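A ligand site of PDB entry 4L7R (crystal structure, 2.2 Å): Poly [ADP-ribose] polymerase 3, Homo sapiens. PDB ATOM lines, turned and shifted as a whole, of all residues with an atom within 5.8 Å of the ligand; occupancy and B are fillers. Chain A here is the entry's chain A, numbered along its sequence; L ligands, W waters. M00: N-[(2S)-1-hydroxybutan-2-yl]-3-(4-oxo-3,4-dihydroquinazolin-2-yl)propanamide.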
ATOM      1  N   LYS A 108     -30.485 -21.375 -16.818  1.00  0.00           N
ATOM      2  CA  LYS A 108     -30.202 -21.167 -15.390  1.00  0.00           C
ATOM      3  C   LYS A 108     -29.038 -20.204 -15.243  1.00  0.00           C
ATOM      4  O   LYS A 108     -29.105 -19.301 -14.413  1.00  0.00           O
ATOM      5  CB  LYS A 108     -29.893 -22.492 -14.684  1.00  0.00           C
ATOM      6  CG  LYS A 108     -31.108 -23.381 -14.460  1.00  0.00           C
ATOM      7  CD  LYS A 108     -30.720 -24.696 -13.771  1.00  0.00           C
ATOM      8  CE  LYS A 108     -31.883 -25.637 -13.650  1.00  0.00           C
ATOM      9  NZ  LYS A 108     -31.586 -26.765 -12.734  1.00  0.00           N
ATOM     10  N   ASP A 109     -27.982 -20.392 -16.050  1.00  0.00           N
ATOM     11  CA  ASP A 109     -26.748 -19.581 -16.093  1.00  0.00           C
ATOM     12  C   ASP A 109     -27.065 -18.153 -16.516  1.00  0.00           C
ATOM     13  O   ASP A 109     -26.482 -17.221 -15.960  1.00  0.00           O
ATOM     14  CB  ASP A 109     -25.718 -20.216 -17.054  1.00  0.00           C
ATOM     15  CG  ASP A 109     -25.082 -21.491 -16.518  1.00  0.00           C
ATOM     16  OD1 ASP A 109     -25.294 -21.815 -15.314  1.00  0.00           O
ATOM     17  OD2 ASP A 109     -24.377 -22.171 -17.297  1.00  0.00           O
ATOM     18  N   LEU A 112     -28.639 -16.505 -13.499  1.00  0.00           N
ATOM     19  CA  LEU A 112     -27.656 -16.268 -12.436  1.00  0.00           C
ATOM     20  C   LEU A 112     -26.934 -14.945 -12.685  1.00  0.00           C
ATOM     21  O   LEU A 112     -26.668 -14.185 -11.739  1.00  0.00           O
ATOM     22  CB  LEU A 112     -26.657 -17.433 -12.313  1.00  0.00           C
ATOM     23  CG  LEU A 112     -27.210 -18.742 -11.706  1.00  0.00           C
ATOM     24  CD1 LEU A 112     -26.256 -19.896 -11.969  1.00  0.00           C
ATOM     25  CD2 LEU A 112     -27.450 -18.605 -10.214  1.00  0.00           C
ATOM     26  N   VAL A 113     -26.692 -14.653 -13.974  1.00  0.00           N
ATOM     27  CA  VAL A 113     -26.088 -13.397 -14.415  1.00  0.00           C
ATOM     28  C   VAL A 113     -27.108 -12.271 -14.185  1.00  0.00           C
ATOM     29  O   VAL A 113     -26.757 -11.210 -13.664  1.00  0.00           O
ATOM     30  CB  VAL A 113     -25.639 -13.478 -15.908  1.00  0.00           C
ATOM     31  CG1 VAL A 113     -25.124 -12.112 -16.393  1.00  0.00           C
ATOM     32  CG2 VAL A 113     -24.582 -14.584 -16.098  1.00  0.00           C
ATOM     33  N   ASP A 116     -27.311 -11.224 -10.674  1.00  0.00           N
ATOM     34  CA  ASP A 116     -26.160 -10.396 -10.291  1.00  0.00           C
ATOM     35  C   ASP A 116     -26.297  -8.987 -10.865  1.00  0.00           C
ATOM     36  O   ASP A 116     -25.708  -8.048 -10.320  1.00  0.00           O
ATOM     37  CB  ASP A 116     -24.831 -11.049 -10.727  1.00  0.00           C
ATOM     38  CG  ASP A 116     -24.281 -12.108  -9.754  1.00  0.00           C
ATOM     39  OD1 ASP A 116     -24.792 -12.211  -8.610  1.00  0.00           O
ATOM     40  OD2 ASP A 116     -23.302 -12.786 -10.117  1.00  0.00           O
ATOM     41  N   TRP A 208      -7.230 -18.714 -11.597  1.00  0.00           N
ATOM     42  CA  TRP A 208      -8.060 -17.816 -12.388  1.00  0.00           C
ATOM     43  C   TRP A 208      -9.568 -18.100 -12.218  1.00  0.00           C
ATOM     44  O   TRP A 208      -9.984 -19.250 -12.121  1.00  0.00           O
ATOM     45  CB  TRP A 208      -7.710 -17.958 -13.880  1.00  0.00           C
ATOM     46  CG  TRP A 208      -6.279 -17.684 -14.187  1.00  0.00           C
ATOM     47  CD1 TRP A 208      -5.299 -18.597 -14.446  1.00  0.00           C
ATOM     48  CD2 TRP A 208      -5.660 -16.394 -14.292  1.00  0.00           C
ATOM     49  NE1 TRP A 208      -4.126 -17.952 -14.738  1.00  0.00           N
ATOM     50  CE2 TRP A 208      -4.293 -16.606 -14.581  1.00  0.00           C
ATOM     51  CE3 TRP A 208      -6.118 -15.075 -14.086  1.00  0.00           C
ATOM     52  CZ2 TRP A 208      -3.388 -15.553 -14.733  1.00  0.00           C
ATOM     53  CZ3 TRP A 208      -5.203 -14.033 -14.213  1.00  0.00           C
ATOM     54  CH2 TRP A 208      -3.851 -14.277 -14.509  1.00  0.00           C
ATOM     55  N   HIS A 209     -10.377 -17.021 -12.294  1.00  0.00           N
ATOM     56  CA  HIS A 209     -11.822 -17.087 -12.285  1.00  0.00           C
ATOM     57  C   HIS A 209     -12.311 -15.973 -13.211  1.00  0.00           C
ATOM     58  O   HIS A 209     -12.260 -14.782 -12.861  1.00  0.00           O
ATOM     59  CB  HIS A 209     -12.433 -16.997 -10.862  1.00  0.00           C
ATOM     60  CG  HIS A 209     -13.923 -17.150 -10.875  1.00  0.00           C
ATOM     61  ND1 HIS A 209     -14.513 -18.401 -10.857  1.00  0.00           N
ATOM     62  CD2 HIS A 209     -14.889 -16.210 -10.972  1.00  0.00           C
ATOM     63  CE1 HIS A 209     -15.819 -18.177 -10.927  1.00  0.00           C
ATOM     64  NE2 HIS A 209     -16.089 -16.884 -11.008  1.00  0.00           N
ATOM     65  N   GLY A 210     -12.682 -16.367 -14.418  1.00  0.00           N
ATOM     66  CA  GLY A 210     -13.144 -15.420 -15.430  1.00  0.00           C
ATOM     67  C   GLY A 210     -14.663 -15.330 -15.439  1.00  0.00           C
ATOM     68  O   GLY A 210     -15.342 -16.337 -15.240  1.00  0.00           O
ATOM     69  N   THR A 211     -15.209 -14.116 -15.630  1.00  0.00           N
ATOM     70  CA  THR A 211     -16.656 -13.868 -15.679  1.00  0.00           C
ATOM     71  C   THR A 211     -16.952 -12.771 -16.668  1.00  0.00           C
ATOM     72  O   THR A 211     -16.035 -12.077 -17.091  1.00  0.00           O
ATOM     73  CB  THR A 211     -17.225 -13.434 -14.317  1.00  0.00           C
ATOM     74  OG1 THR A 211     -16.778 -12.111 -13.987  1.00  0.00           O
ATOM     75  CG2 THR A 211     -16.953 -14.401 -13.190  1.00  0.00           C
ATOM     76  N   ASN A 212     -18.232 -12.544 -16.957  1.00  0.00           N
ATOM     77  CA  ASN A 212     -18.543 -11.381 -17.770  1.00  0.00           C
ATOM     78  C   ASN A 212     -18.550 -10.142 -16.825  1.00  0.00           C
ATOM     79  O   ASN A 212     -18.585 -10.265 -15.580  1.00  0.00           O
ATOM     80  CB  ASN A 212     -19.816 -11.549 -18.591  1.00  0.00           C
ATOM     81  CG  ASN A 212     -21.013 -12.017 -17.835  1.00  0.00           C
ATOM     82  OD1 ASN A 212     -21.519 -11.319 -16.941  1.00  0.00           O
ATOM     83  ND2 ASN A 212     -21.478 -13.194 -18.186  1.00  0.00           N
ATOM     84  N   VAL A 215     -21.194  -9.200 -13.760  1.00  0.00           N
ATOM     85  CA  VAL A 215     -21.240  -9.878 -12.456  1.00  0.00           C
ATOM     86  C   VAL A 215     -20.070  -9.416 -11.532  1.00  0.00           C
ATOM     87  O   VAL A 215     -20.040  -9.822 -10.358  1.00  0.00           O
ATOM     88  CB  VAL A 215     -21.304 -11.433 -12.544  1.00  0.00           C
ATOM     89  CG1 VAL A 215     -22.491 -11.913 -13.352  1.00  0.00           C
ATOM     90  CG2 VAL A 215     -20.021 -12.028 -13.087  1.00  0.00           C
ATOM     91  N   ILE A 219     -19.648  -9.752  -7.411  1.00  0.00           N
ATOM     92  CA  ILE A 219     -18.557 -10.545  -6.855  1.00  0.00           C
ATOM     93  C   ILE A 219     -17.731  -9.686  -5.881  1.00  0.00           C
ATOM     94  O   ILE A 219     -17.340 -10.192  -4.841  1.00  0.00           O
ATOM     95  CB  ILE A 219     -17.680 -11.198  -7.961  1.00  0.00           C
ATOM     96  CG1 ILE A 219     -18.490 -12.291  -8.695  1.00  0.00           C
ATOM     97  CG2 ILE A 219     -16.376 -11.765  -7.401  1.00  0.00           C
ATOM     98  CD1 ILE A 219     -17.895 -12.653 -10.081  1.00  0.00           C
ATOM     99  N   SER A 230     -26.949 -23.344  -9.634  1.00  0.00           N
ATOM    100  CA  SER A 230     -25.658 -23.363 -10.343  1.00  0.00           C
ATOM    101  C   SER A 230     -25.207 -24.819 -10.572  1.00  0.00           C
ATOM    102  O   SER A 230     -25.700 -25.740  -9.909  1.00  0.00           O
ATOM    103  CB  SER A 230     -24.594 -22.545  -9.613  1.00  0.00           C
ATOM    104  OG  SER A 230     -24.153 -23.138  -8.410  1.00  0.00           O
ATOM    105  N   TYR A 239     -15.877 -22.732  -9.664  1.00  0.00           N
ATOM    106  CA  TYR A 239     -14.998 -23.157 -10.750  1.00  0.00           C
ATOM    107  C   TYR A 239     -13.798 -22.235 -10.953  1.00  0.00           C
ATOM    108  O   TYR A 239     -13.944 -21.024 -11.144  1.00  0.00           O
ATOM    109  CB  TYR A 239     -15.799 -23.250 -12.056  1.00  0.00           C
ATOM    110  CG  TYR A 239     -16.729 -24.441 -12.107  1.00  0.00           C
ATOM    111  CD1 TYR A 239     -17.965 -24.414 -11.464  1.00  0.00           C
ATOM    112  CD2 TYR A 239     -16.435 -25.543 -12.920  1.00  0.00           C
ATOM    113  CE1 TYR A 239     -18.837 -25.513 -11.521  1.00  0.00           C
ATOM    114  CE2 TYR A 239     -17.318 -26.631 -13.003  1.00  0.00           C
ATOM    115  CZ  TYR A 239     -18.508 -26.600 -12.307  1.00  0.00           C
ATOM    116  OH  TYR A 239     -19.365 -27.671 -12.393  1.00  0.00           O
ATOM    117  N   PHE A 240     -12.620 -22.840 -10.978  1.00  0.00           N
ATOM    118  CA  PHE A 240     -11.357 -22.146 -11.203  1.00  0.00           C
ATOM    119  C   PHE A 240     -10.532 -22.854 -12.242  1.00  0.00           C
ATOM    120  O   PHE A 240     -10.762 -24.029 -12.525  1.00  0.00           O
ATOM    121  CB  PHE A 240     -10.545 -22.059  -9.904  1.00  0.00           C
ATOM    122  CG  PHE A 240     -11.162 -21.264  -8.794  1.00  0.00           C
ATOM    123  CD1 PHE A 240     -10.940 -19.896  -8.690  1.00  0.00           C
ATOM    124  CD2 PHE A 240     -11.898 -21.896  -7.796  1.00  0.00           C
ATOM    125  CE1 PHE A 240     -11.505 -19.158  -7.650  1.00  0.00           C
ATOM    126  CE2 PHE A 240     -12.434 -21.164  -6.735  1.00  0.00           C
ATOM    127  CZ  PHE A 240     -12.233 -19.801  -6.672  1.00  0.00           C
ATOM    128  N   ALA A 241      -9.564 -22.141 -12.818  1.00  0.00           N
ATOM    129  CA  ALA A 241      -8.628 -22.720 -13.786  1.00  0.00           C
ATOM    130  C   ALA A 241      -7.198 -22.270 -13.464  1.00  0.00           C
ATOM    131  O   ALA A 241      -7.017 -21.174 -12.976  1.00  0.00           O
ATOM    132  CB  ALA A 241      -8.992 -22.323 -15.202  1.00  0.00           C
ATOM    133  N   LYS A 246      -8.410 -20.802 -20.274  1.00  0.00           N
ATOM    134  CA  LYS A 246      -9.647 -21.487 -19.903  1.00  0.00           C
ATOM    135  C   LYS A 246     -10.608 -20.465 -19.253  1.00  0.00           C
ATOM    136  O   LYS A 246     -11.766 -20.386 -19.658  1.00  0.00           O
ATOM    137  CB  LYS A 246      -9.369 -22.690 -18.979  1.00  0.00           C
ATOM    138  CG  LYS A 246     -10.616 -23.419 -18.459  1.00  0.00           C
ATOM    139  CD  LYS A 246     -11.573 -23.856 -19.565  1.00  0.00           C
ATOM    140  CE  LYS A 246     -12.832 -24.486 -19.020  1.00  0.00           C
ATOM    141  NZ  LYS A 246     -13.830 -24.665 -20.109  1.00  0.00           N
ATOM    142  N   SER A 247     -10.115 -19.661 -18.297  1.00  0.00           N
ATOM    143  CA  SER A 247     -10.947 -18.639 -17.652  1.00  0.00           C
ATOM    144  C   SER A 247     -11.313 -17.457 -18.563  1.00  0.00           C
ATOM    145  O   SER A 247     -12.362 -16.847 -18.376  1.00  0.00           O
ATOM    146  CB  SER A 247     -10.291 -18.131 -16.381  1.00  0.00           C
ATOM    147  OG  SER A 247     -10.333 -19.182 -15.433  1.00  0.00           O
ATOM    148  N   ALA A 248     -10.457 -17.140 -19.552  1.00  0.00           N
ATOM    149  CA  ALA A 248     -10.662 -16.018 -20.495  1.00  0.00           C
ATOM    150  C   ALA A 248     -11.855 -16.272 -21.434  1.00  0.00           C
ATOM    151  O   ALA A 248     -12.511 -15.317 -21.838  1.00  0.00           O
ATOM    152  CB  ALA A 248      -9.402 -15.754 -21.322  1.00  0.00           C
ATOM    153  N   TYR A 250     -14.684 -17.154 -20.668  1.00  0.00           N
ATOM    154  CA  TYR A 250     -15.877 -16.687 -19.939  1.00  0.00           C
ATOM    155  C   TYR A 250     -15.949 -15.172 -19.837  1.00  0.00           C
ATOM    156  O   TYR A 250     -16.930 -14.624 -19.309  1.00  0.00           O
ATOM    157  CB  TYR A 250     -15.918 -17.333 -18.540  1.00  0.00           C
ATOM    158  CG  TYR A 250     -15.969 -18.842 -18.648  1.00  0.00           C
ATOM    159  CD1 TYR A 250     -17.152 -19.504 -18.967  1.00  0.00           C
ATOM    160  CD2 TYR A 250     -14.807 -19.603 -18.550  1.00  0.00           C
ATOM    161  CE1 TYR A 250     -17.187 -20.881 -19.150  1.00  0.00           C
ATOM    162  CE2 TYR A 250     -14.829 -20.990 -18.731  1.00  0.00           C
ATOM    163  CZ  TYR A 250     -16.016 -21.626 -19.037  1.00  0.00           C
ATOM    164  OH  TYR A 250     -16.071 -22.999 -19.210  1.00  0.00           O
ATOM    165  N   SER A 338      -7.546 -28.257 -16.993  1.00  0.00           N
ATOM    166  CA  SER A 338      -7.968 -28.498 -15.597  1.00  0.00           C
ATOM    167  C   SER A 338      -9.033 -27.517 -15.098  1.00  0.00           C
ATOM    168  O   SER A 338      -9.004 -26.317 -15.412  1.00  0.00           O
ATOM    169  CB  SER A 338      -6.786 -28.439 -14.636  1.00  0.00           C
ATOM    170  OG  SER A 338      -5.919 -29.555 -14.824  1.00  0.00           O
ATOM    171  N   GLU A 339      -9.951 -28.044 -14.294  1.00  0.00           N
ATOM    172  CA  GLU A 339     -10.987 -27.287 -13.615  1.00  0.00           C
ATOM    173  C   GLU A 339     -10.880 -27.598 -12.138  1.00  0.00           C
ATOM    174  O   GLU A 339     -10.977 -28.764 -11.757  1.00  0.00           O
ATOM    175  CB  GLU A 339     -12.392 -27.622 -14.153  1.00  0.00           C
ATOM    176  CG  GLU A 339     -12.586 -27.276 -15.638  1.00  0.00           C
ATOM    177  CD  GLU A 339     -14.008 -27.477 -16.132  1.00  0.00           C
ATOM    178  OE1 GLU A 339     -14.929 -27.595 -15.284  1.00  0.00           O
ATOM    179  OE2 GLU A 339     -14.221 -27.483 -17.358  1.00  0.00           O
ATOM    180  N   TYR A 340     -10.621 -26.562 -11.311  1.00  0.00           N
ATOM    181  CA  TYR A 340     -10.449 -26.681  -9.856  1.00  0.00           C
ATOM    182  C   TYR A 340     -11.743 -26.284  -9.175  1.00  0.00           C
ATOM    183  O   TYR A 340     -12.310 -25.214  -9.446  1.00  0.00           O
ATOM    184  CB  TYR A 340      -9.287 -25.800  -9.371  1.00  0.00           C
ATOM    185  CG  TYR A 340      -7.918 -26.264  -9.809  1.00  0.00           C
ATOM    186  CD1 TYR A 340      -7.517 -26.157 -11.152  1.00  0.00           C
ATOM    187  CD2 TYR A 340      -6.983 -26.706  -8.879  1.00  0.00           C
ATOM    188  CE1 TYR A 340      -6.240 -26.565 -11.550  1.00  0.00           C
ATOM    189  CE2 TYR A 340      -5.700 -27.094  -9.271  1.00  0.00           C
ATOM    190  CZ  TYR A 340      -5.337 -27.030 -10.606  1.00  0.00           C
ATOM    191  OH  TYR A 340      -4.075 -27.406 -10.984  1.00  0.00           O
HETATM  192  CAA M00 L   1     -23.469 -19.049 -13.961  1.00  0.00           C
HETATM  193  CAI M00 L   1     -22.737 -18.268 -15.007  1.00  0.00           C
HETATM  194  CAU M00 L   1     -21.802 -17.283 -14.290  1.00  0.00           C
HETATM  195  CAJ M00 L   1     -22.373 -16.519 -13.083  1.00  0.00           C
HETATM  196  OAD M00 L   1     -21.252 -15.701 -12.622  1.00  0.00           O
HETATM  197  NAN M00 L   1     -20.485 -17.971 -13.977  1.00  0.00           N
HETATM  198  CAP M00 L   1     -19.332 -17.613 -14.577  1.00  0.00           C
HETATM  199  OAB M00 L   1     -19.241 -16.694 -15.453  1.00  0.00           O
HETATM  200  CAK M00 L   1     -18.156 -18.454 -14.077  1.00  0.00           C
HETATM  201  CAL M00 L   1     -17.625 -19.062 -15.337  1.00  0.00           C
HETATM  202  CAQ M00 L   1     -16.416 -19.734 -15.242  1.00  0.00           C
HETATM  203  NAM M00 L   1     -16.480 -21.069 -15.406  1.00  0.00           N
HETATM  204  CAS M00 L   1     -15.362 -21.809 -15.363  1.00  0.00           C
HETATM  205  CAG M00 L   1     -15.488 -23.169 -15.584  1.00  0.00           C
HETATM  206  CAE M00 L   1     -14.321 -23.927 -15.580  1.00  0.00           C
HETATM  207  CAF M00 L   1     -13.110 -23.363 -15.304  1.00  0.00           C
HETATM  208  CAH M00 L   1     -12.946 -21.991 -15.094  1.00  0.00           C
HETATM  209  CAT M00 L   1     -14.051 -21.177 -15.121  1.00  0.00           C
HETATM  210  CAR M00 L   1     -13.970 -19.778 -14.946  1.00  0.00           C
HETATM  211  OAC M00 L   1     -12.912 -19.148 -14.802  1.00  0.00           O
HETATM  212  NAO M00 L   1     -15.165 -19.101 -15.022  1.00  0.00           N
HETATM  213  O   HOH W   1     -18.958 -16.360 -11.022  1.00  0.00           O
HETATM  214  O   HOH W   2     -23.423 -22.349 -13.030  1.00  0.00           O
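Water W1 lies within hydrogen-bond range of OAD of the ligand (2.9 Å) and NE2 of His 209 (2.9 Å).
Merely in contact with the ligand: Asp 109, Leu 112, Trp 208, His 209, Thr 211, Val 215, Tyr 239, Phe 240, Ala 241, Lys 246, Tyr 250 and Glu 339. Of the 23 residues printed, 14 come within 4 Å of the ligand. The nearest printed residue that does not touch the ligand is Val 113 (4.2 Å).
The side-chain hydroxyl of Ser 247 is in hydrogen-bond range of an oxygen (OAC) of the ligand. The backbone NH (N) of Gly 210 lies within hydrogen-bond range of an oxygen (OAC) of the ligand, at 2.8 Å. A nitrogen (NAO) of the ligand sits at hydrogen-bond distance from the backbone carbonyl oxygen (O) of Gly 210 (2.8 Å).
OG of Ser 247 sits close to O of Trp 208 (3.3 Å). O of Tyr 239 is in hydrogen-bond range of ND1 of His 209, at 2.7 Å. NZ of Lys 246 sits at hydrogen-bond distance from OH of Tyr 250 (2.9 Å). The backbone NH (N) of Asn 212 lies within hydrogen-bond range of the backbone carbonyl oxygen (O) of Tyr 250 (3.4 Å). OE2 of Glu 339 is in salt-bridge range of NZ of Lys 246 (3.96 Å). N of Tyr 340 is in hydrogen-bond range of O of Phe 240, at 2.8 Å. The backbone NH (N) of Trp 208 sits at hydrogen-bond distance from the backbone carbonyl oxygen (O) of Ala 241, 2.8 Å away.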
